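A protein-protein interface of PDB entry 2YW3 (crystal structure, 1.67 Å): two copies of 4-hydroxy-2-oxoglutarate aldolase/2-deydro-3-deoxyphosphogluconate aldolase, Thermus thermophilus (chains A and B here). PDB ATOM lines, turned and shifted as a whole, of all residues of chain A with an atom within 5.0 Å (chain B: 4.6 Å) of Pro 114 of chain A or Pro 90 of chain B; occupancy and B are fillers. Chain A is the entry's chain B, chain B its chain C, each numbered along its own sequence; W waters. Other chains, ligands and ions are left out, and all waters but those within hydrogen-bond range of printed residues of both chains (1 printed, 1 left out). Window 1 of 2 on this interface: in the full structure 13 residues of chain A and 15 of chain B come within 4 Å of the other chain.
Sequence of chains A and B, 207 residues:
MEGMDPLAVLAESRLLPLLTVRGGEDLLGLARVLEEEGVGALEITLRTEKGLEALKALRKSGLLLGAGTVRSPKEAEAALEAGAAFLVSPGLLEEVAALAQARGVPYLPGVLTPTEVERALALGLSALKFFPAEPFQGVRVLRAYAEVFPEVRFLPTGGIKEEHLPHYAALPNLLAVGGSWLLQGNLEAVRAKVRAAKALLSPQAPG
Pro 114 of chain A touches Pro 90 of chain B. Pro 114 of chain A touches Gly 91 of chain B. CD1 of Leu 112 of chain B touches CD of Pro 114 of chain A, at 3.5 Å. Pro 114 of chain A touches Phe 131 of chain B. CA of Gly 91 of chain B touches OG1 of Thr 115 of chain A, at 3.4 Å. O of Gly 110 of chain B touches OG1 of Thr 115 of chain A (3.7 Å). Val 148 of chain A touches Thr 69 of chain B. Val 148 of chain A touches Phe 131 of chain B. Phe 149 of chain A touches Arg 71 of chain B (CD1 to NH2, 3.3 Å). CZ of Phe 149 of chain A touches CB of Pro 90 of chain B, at 3.9 Å.
Position printed for both chains: 112.
Pro 114 of chain A touches four residues of chain B. Printed residues of chain A within 4 Å of Pro 90 of chain B: Pro 114 and Phe 149. Of the printed residues of chain A, Leu 112 of chain B touches Pro 114 (3.5 Å). Of the printed residues of chain B, Val 148 of chain A touches Thr 69, Arg 71 and Phe 131.
The backbone NH (N) of Gly 110 of chain B lies within hydrogen-bond range of the backbone carbonyl oxygen (O) of Ser 89 of chain B (3.0 Å). The backbone carbonyl oxygen of Gly 91 of chain B is in hydrogen-bond range of the side-chain hydroxyl of Ser 89 of chain B (2.5 Å). The backbone NH (N) of Thr 115 of chain A sits close to the side-chain hydroxyl (OG1) of Thr 113 of chain A (3.4 Å). The backbone NH of Thr 69 of chain B lies within hydrogen-bond range of the backbone carbonyl oxygen of Val 88 of chain B (3.4 Å).
Water W1 lies within hydrogen-bond range of OG1 of Thr 115 of chain A and O of Gly 110 of chain B.
The side-chain carboxylate (OE2) of Glu 118 of chain A is in salt-bridge range of the guanidinium group (NE) of Arg 71 of chain B (2.6 Å). NH1 of Arg 71 of chain B sits at hydrogen-bond distance from O of Val 148 of chain A.
Of the 10 printed residues of chain A, 5 touch a printed residue of chain B. Printed residues of chain A that touch a printed residue of chain B: Pro 114, Thr 115, Glu 118, Val 148 and Phe 149. Hydrophobic or aromatic side chains of chain A within 4 Å of the printed part of chain B: Pro 114, Val 148 and Phe 149. Along chain A the printed residues that touch a printed residue of chain B span positions 114 to 149. Hydrophobic or aromatic side chains of chain B within 4 Å of the printed part of chain A: Pro 90, Leu 112 and Phe 131. Along chain B the printed residues that touch a printed residue of chain A span positions 69 to 131.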
ATOM      1  N   LEU A 112      12.687  -4.718  19.471  1.00  0.00           N
ATOM      2  CA  LEU A 112      13.669  -4.190  20.430  1.00  0.00           C
ATOM      3  C   LEU A 112      14.912  -5.069  20.534  1.00  0.00           C
ATOM      4  O   LEU A 112      16.042  -4.566  20.538  1.00  0.00           O
ATOM      5  CB  LEU A 112      13.051  -4.087  21.815  1.00  0.00           C
ATOM      6  CG  LEU A 112      12.112  -2.912  22.040  1.00  0.00           C
ATOM      7  CD1 LEU A 112      11.373  -3.142  23.341  1.00  0.00           C
ATOM      8  CD2 LEU A 112      12.920  -1.542  22.069  1.00  0.00           C
ATOM      9  N   THR A 113      14.713  -6.390  20.645  1.00  0.00           N
ATOM     10  CA  THR A 113      15.830  -7.276  21.006  1.00  0.00           C
ATOM     11  C   THR A 113      16.452  -7.926  19.768  1.00  0.00           C
ATOM     12  O   THR A 113      15.812  -8.005  18.725  1.00  0.00           O
ATOM     13  CB  THR A 113      15.367  -8.428  21.911  1.00  0.00           C
ATOM     14  OG1 THR A 113      14.570  -9.362  21.140  1.00  0.00           O
ATOM     15  CG2 THR A 113      14.535  -7.915  23.128  1.00  0.00           C
ATOM     16  N   PRO A 114      17.698  -8.401  19.886  1.00  0.00           N
ATOM     17  CA  PRO A 114      18.332  -9.093  18.733  1.00  0.00           C
ATOM     18  C   PRO A 114      17.510 -10.286  18.242  1.00  0.00           C
ATOM     19  O   PRO A 114      17.483 -10.553  17.041  1.00  0.00           O
ATOM     20  CB  PRO A 114      19.651  -9.565  19.320  1.00  0.00           C
ATOM     21  CG  PRO A 114      19.968  -8.470  20.355  1.00  0.00           C
ATOM     22  CD  PRO A 114      18.634  -8.296  21.022  1.00  0.00           C
ATOM     23  N   THR A 115      16.834 -10.992  19.138  1.00  0.00           N
ATOM     24  CA  THR A 115      16.018 -12.166  18.715  1.00  0.00           C
ATOM     25  C   THR A 115      14.888 -11.680  17.829  1.00  0.00           C
ATOM     26  O   THR A 115      14.544 -12.299  16.819  1.00  0.00           O
ATOM     27  CB  THR A 115      15.533 -12.923  19.952  1.00  0.00           C
ATOM     28  OG1 THR A 115      16.671 -13.422  20.661  1.00  0.00           O
ATOM     29  CG2 THR A 115      14.609 -14.104  19.612  1.00  0.00           C
ATOM     30  N   GLU A 116      14.302 -10.534  18.211  1.00  0.00           N
ATOM     31  CA  GLU A 116      13.200  -9.946  17.448  1.00  0.00           C
ATOM     32  C   GLU A 116      13.699  -9.442  16.093  1.00  0.00           C
ATOM     33  O   GLU A 116      13.007  -9.588  15.085  1.00  0.00           O
ATOM     34  CB  GLU A 116      12.527  -8.829  18.257  1.00  0.00           C
ATOM     35  CG  GLU A 116      11.739  -9.417  19.433  1.00  0.00           C
ATOM     36  CD  GLU A 116      11.284  -8.380  20.482  1.00  0.00           C
ATOM     37  OE1 GLU A 116      11.704  -7.187  20.406  1.00  0.00           O
ATOM     38  OE2 GLU A 116      10.502  -8.805  21.373  1.00  0.00           O
ATOM     39  N   VAL A 117      14.900  -8.860  16.056  1.00  0.00           N
ATOM     40  CA  VAL A 117      15.489  -8.433  14.771  1.00  0.00           C
ATOM     41  C   VAL A 117      15.631  -9.669  13.862  1.00  0.00           C
ATOM     42  O   VAL A 117      15.237  -9.657  12.687  1.00  0.00           O
ATOM     43  CB  VAL A 117      16.834  -7.751  14.970  1.00  0.00           C
ATOM     44  CG1 VAL A 117      17.545  -7.488  13.618  1.00  0.00           C
ATOM     45  CG2 VAL A 117      16.641  -6.417  15.760  1.00  0.00           C
ATOM     46  N   GLU A 118      16.179 -10.738  14.419  1.00  0.00           N
ATOM     47  CA  GLU A 118      16.401 -11.947  13.603  1.00  0.00           C
ATOM     48  C   GLU A 118      15.074 -12.511  13.100  1.00  0.00           C
ATOM     49  O   GLU A 118      14.990 -12.978  11.950  1.00  0.00           O
ATOM     50  CB  GLU A 118      17.212 -12.999  14.356  1.00  0.00           C
ATOM     51  CG  GLU A 118      18.663 -12.603  14.675  1.00  0.00           C
ATOM     52  CD  GLU A 118      19.628 -12.706  13.480  1.00  0.00           C
ATOM     53  OE1 GLU A 118      19.198 -12.465  12.328  1.00  0.00           O
ATOM     54  OE2 GLU A 118      20.830 -13.005  13.690  1.00  0.00           O
ATOM     55  N   TYR A 145      23.731  -2.470  17.249  1.00  0.00           N
ATOM     56  CA  TYR A 145      23.092  -3.178  16.128  1.00  0.00           C
ATOM     57  C   TYR A 145      23.724  -2.813  14.792  1.00  0.00           C
ATOM     58  O   TYR A 145      23.671  -3.609  13.859  1.00  0.00           O
ATOM     59  CB  TYR A 145      21.590  -2.915  16.081  1.00  0.00           C
ATOM     60  CG  TYR A 145      20.822  -3.539  17.216  1.00  0.00           C
ATOM     61  CD1 TYR A 145      21.469  -4.311  18.207  1.00  0.00           C
ATOM     62  CD2 TYR A 145      19.443  -3.371  17.302  1.00  0.00           C
ATOM     63  CE1 TYR A 145      20.738  -4.899  19.252  1.00  0.00           C
ATOM     64  CE2 TYR A 145      18.690  -3.971  18.355  1.00  0.00           C
ATOM     65  CZ  TYR A 145      19.353  -4.720  19.313  1.00  0.00           C
ATOM     66  OH  TYR A 145      18.630  -5.282  20.347  1.00  0.00           O
ATOM     67  N   VAL A 148      26.480  -5.541  14.469  1.00  0.00           N
ATOM     68  CA  VAL A 148      26.035  -6.931  14.331  1.00  0.00           C
ATOM     69  C   VAL A 148      24.918  -7.148  13.291  1.00  0.00           C
ATOM     70  O   VAL A 148      24.762  -8.261  12.784  1.00  0.00           O
ATOM     71  CB  VAL A 148      25.656  -7.613  15.711  1.00  0.00           C
ATOM     72  CG1 VAL A 148      26.817  -7.498  16.698  1.00  0.00           C
ATOM     73  CG2 VAL A 148      24.430  -7.008  16.316  1.00  0.00           C
ATOM     74  N   PHE A 149      24.155  -6.107  12.966  1.00  0.00           N
ATOM     75  CA  PHE A 149      23.108  -6.211  11.943  1.00  0.00           C
ATOM     76  C   PHE A 149      23.291  -5.121  10.897  1.00  0.00           C
ATOM     77  O   PHE A 149      22.433  -4.256  10.746  1.00  0.00           O
ATOM     78  CB  PHE A 149      21.679  -6.057  12.517  1.00  0.00           C
ATOM     79  CG  PHE A 149      21.309  -7.080  13.593  1.00  0.00           C
ATOM     80  CD1 PHE A 149      21.213  -8.435  13.300  1.00  0.00           C
ATOM     81  CD2 PHE A 149      21.019  -6.666  14.888  1.00  0.00           C
ATOM     82  CE1 PHE A 149      20.853  -9.380  14.293  1.00  0.00           C
ATOM     83  CE2 PHE A 149      20.636  -7.575  15.879  1.00  0.00           C
ATOM     84  CZ  PHE A 149      20.558  -8.968  15.586  1.00  0.00           C
ATOM     85  N   THR B  69      28.610 -13.529  16.069  1.00  0.00           N
ATOM     86  CA  THR B  69      27.778 -12.942  15.047  1.00  0.00           C
ATOM     87  C   THR B  69      27.292 -14.024  14.073  1.00  0.00           C
ATOM     88  O   THR B  69      27.085 -13.745  12.896  1.00  0.00           O
ATOM     89  CB  THR B  69      28.503 -11.794  14.281  1.00  0.00           C
ATOM     90  OG1 THR B  69      29.371 -11.090  15.188  1.00  0.00           O
ATOM     91  CG2 THR B  69      27.507 -10.797  13.670  1.00  0.00           C
ATOM     92  N   VAL B  70      27.125 -15.249  14.565  1.00  0.00           N
ATOM     93  CA  VAL B  70      26.594 -16.331  13.726  1.00  0.00           C
ATOM     94  C   VAL B  70      25.140 -15.979  13.378  1.00  0.00           C
ATOM     95  O   VAL B  70      24.345 -15.625  14.266  1.00  0.00           O
ATOM     96  CB  VAL B  70      26.671 -17.688  14.456  1.00  0.00           C
ATOM     97  CG1 VAL B  70      25.910 -18.786  13.694  1.00  0.00           C
ATOM     98  CG2 VAL B  70      28.112 -18.093  14.666  1.00  0.00           C
ATOM     99  N   ARG B  71      24.791 -16.048  12.099  1.00  0.00           N
ATOM    100  CA  ARG B  71      23.479 -15.560  11.665  1.00  0.00           C
ATOM    101  C   ARG B  71      22.604 -16.653  11.039  1.00  0.00           C
ATOM    102  O   ARG B  71      21.424 -16.426  10.779  1.00  0.00           O
ATOM    103  CB  ARG B  71      23.640 -14.405  10.672  1.00  0.00           C
ATOM    104  CG  ARG B  71      24.525 -13.234  11.163  1.00  0.00           C
ATOM    105  CD  ARG B  71      23.886 -12.445  12.336  1.00  0.00           C
ATOM    106  NE  ARG B  71      22.537 -11.993  11.955  1.00  0.00           N
ATOM    107  CZ  ARG B  71      22.266 -10.977  11.134  1.00  0.00           C
ATOM    108  NH1 ARG B  71      23.239 -10.250  10.597  1.00  0.00           N
ATOM    109  NH2 ARG B  71      21.003 -10.690  10.850  1.00  0.00           N
ATOM    110  N   VAL B  88      28.300 -18.493  18.841  1.00  0.00           N
ATOM    111  CA  VAL B  88      27.608 -17.421  19.565  1.00  0.00           C
ATOM    112  C   VAL B  88      26.812 -16.623  18.542  1.00  0.00           C
ATOM    113  O   VAL B  88      27.303 -16.342  17.462  1.00  0.00           O
ATOM    114  CB  VAL B  88      28.633 -16.518  20.281  1.00  0.00           C
ATOM    115  CG1 VAL B  88      27.942 -15.329  20.905  1.00  0.00           C
ATOM    116  CG2 VAL B  88      29.439 -17.333  21.308  1.00  0.00           C
ATOM    117  N   SER B  89      25.569 -16.294  18.857  1.00  0.00           N
ATOM    118  CA  SER B  89      24.755 -15.457  17.958  1.00  0.00           C
ATOM    119  C   SER B  89      24.197 -14.270  18.736  1.00  0.00           C
ATOM    120  O   SER B  89      24.080 -14.336  19.953  1.00  0.00           O
ATOM    121  CB  SER B  89      23.611 -16.263  17.352  1.00  0.00           C
ATOM    122  OG  SER B  89      22.740 -16.747  18.369  1.00  0.00           O
ATOM    123  N   PRO B  90      23.893 -13.155  18.048  1.00  0.00           N
ATOM    124  CA  PRO B  90      23.324 -12.013  18.808  1.00  0.00           C
ATOM    125  C   PRO B  90      21.972 -12.247  19.479  1.00  0.00           C
ATOM    126  O   PRO B  90      21.722 -11.735  20.583  1.00  0.00           O
ATOM    127  CB  PRO B  90      23.197 -10.904  17.744  1.00  0.00           C
ATOM    128  CG  PRO B  90      23.425 -11.559  16.418  1.00  0.00           C
ATOM    129  CD  PRO B  90      24.195 -12.814  16.638  1.00  0.00           C
ATOM    130  N   GLY B  91      21.108 -13.024  18.830  1.00  0.00           N
ATOM    131  CA  GLY B  91      19.840 -13.456  19.445  1.00  0.00           C
ATOM    132  C   GLY B  91      19.636 -14.954  19.304  1.00  0.00           C
ATOM    133  O   GLY B  91      20.508 -15.682  18.868  1.00  0.00           O
ATOM    134  N   GLY B 110      22.350 -15.268  22.205  1.00  0.00           N
ATOM    135  CA  GLY B 110      22.087 -14.046  22.959  1.00  0.00           C
ATOM    136  C   GLY B 110      20.621 -14.002  23.327  1.00  0.00           C
ATOM    137  O   GLY B 110      19.748 -14.306  22.504  1.00  0.00           O
ATOM    138  N   LEU B 112      17.828 -11.489  25.929  1.00  0.00           N
ATOM    139  CA  LEU B 112      17.651 -10.313  26.798  1.00  0.00           C
ATOM    140  C   LEU B 112      16.517 -10.525  27.819  1.00  0.00           C
ATOM    141  O   LEU B 112      16.690 -10.259  29.017  1.00  0.00           O
ATOM    142  CB  LEU B 112      17.414  -9.043  25.979  1.00  0.00           C
ATOM    143  CG  LEU B 112      18.654  -8.430  25.332  1.00  0.00           C
ATOM    144  CD1 LEU B 112      18.291  -7.298  24.411  1.00  0.00           C
ATOM    145  CD2 LEU B 112      19.584  -7.921  26.464  1.00  0.00           C
ATOM    146  N   LYS B 129      24.353 -16.051  26.220  1.00  0.00           N
ATOM    147  CA  LYS B 129      24.911 -14.702  26.111  1.00  0.00           C
ATOM    148  C   LYS B 129      23.810 -13.732  26.525  1.00  0.00           C
ATOM    149  O   LYS B 129      22.647 -13.957  26.204  1.00  0.00           O
ATOM    150  CB  LYS B 129      25.328 -14.439  24.651  1.00  0.00           C
ATOM    151  CG  LYS B 129      25.653 -12.976  24.270  1.00  0.00           C
ATOM    152  CD  LYS B 129      26.508 -12.890  23.018  1.00  0.00           C
ATOM    153  CE  LYS B 129      25.727 -12.428  21.820  1.00  0.00           C
ATOM    154  NZ  LYS B 129      26.658 -11.976  20.728  1.00  0.00           N
ATOM    155  N   PHE B 131      22.947  -9.933  25.683  1.00  0.00           N
ATOM    156  CA  PHE B 131      23.481  -9.027  24.676  1.00  0.00           C
ATOM    157  C   PHE B 131      22.385  -8.180  24.071  1.00  0.00           C
ATOM    158  O   PHE B 131      21.323  -8.715  23.729  1.00  0.00           O
ATOM    159  CB  PHE B 131      24.188  -9.775  23.533  1.00  0.00           C
ATOM    160  CG  PHE B 131      24.519  -8.872  22.353  1.00  0.00           C
ATOM    161  CD1 PHE B 131      25.693  -8.107  22.355  1.00  0.00           C
ATOM    162  CD2 PHE B 131      23.627  -8.735  21.275  1.00  0.00           C
ATOM    163  CE1 PHE B 131      26.001  -7.231  21.277  1.00  0.00           C
ATOM    164  CE2 PHE B 131      23.924  -7.872  20.192  1.00  0.00           C
ATOM    165  CZ  PHE B 131      25.113  -7.110  20.208  1.00  0.00           C
ATOM    166  N   PRO B 132      22.637  -6.860  23.914  1.00  0.00           N
ATOM    167  CA  PRO B 132      23.839  -6.083  24.383  1.00  0.00           C
ATOM    168  C   PRO B 132      23.696  -5.667  25.845  1.00  0.00           C
ATOM    169  O   PRO B 132      22.727  -5.029  26.223  1.00  0.00           O
ATOM    170  CB  PRO B 132      23.863  -4.856  23.470  1.00  0.00           C
ATOM    171  CG  PRO B 132      22.416  -4.731  22.922  1.00  0.00           C
ATOM    172  CD  PRO B 132      21.677  -6.032  23.151  1.00  0.00           C
HETATM  173  O   HOH W   1      16.832 -15.131  22.666  1.00  0.00           O
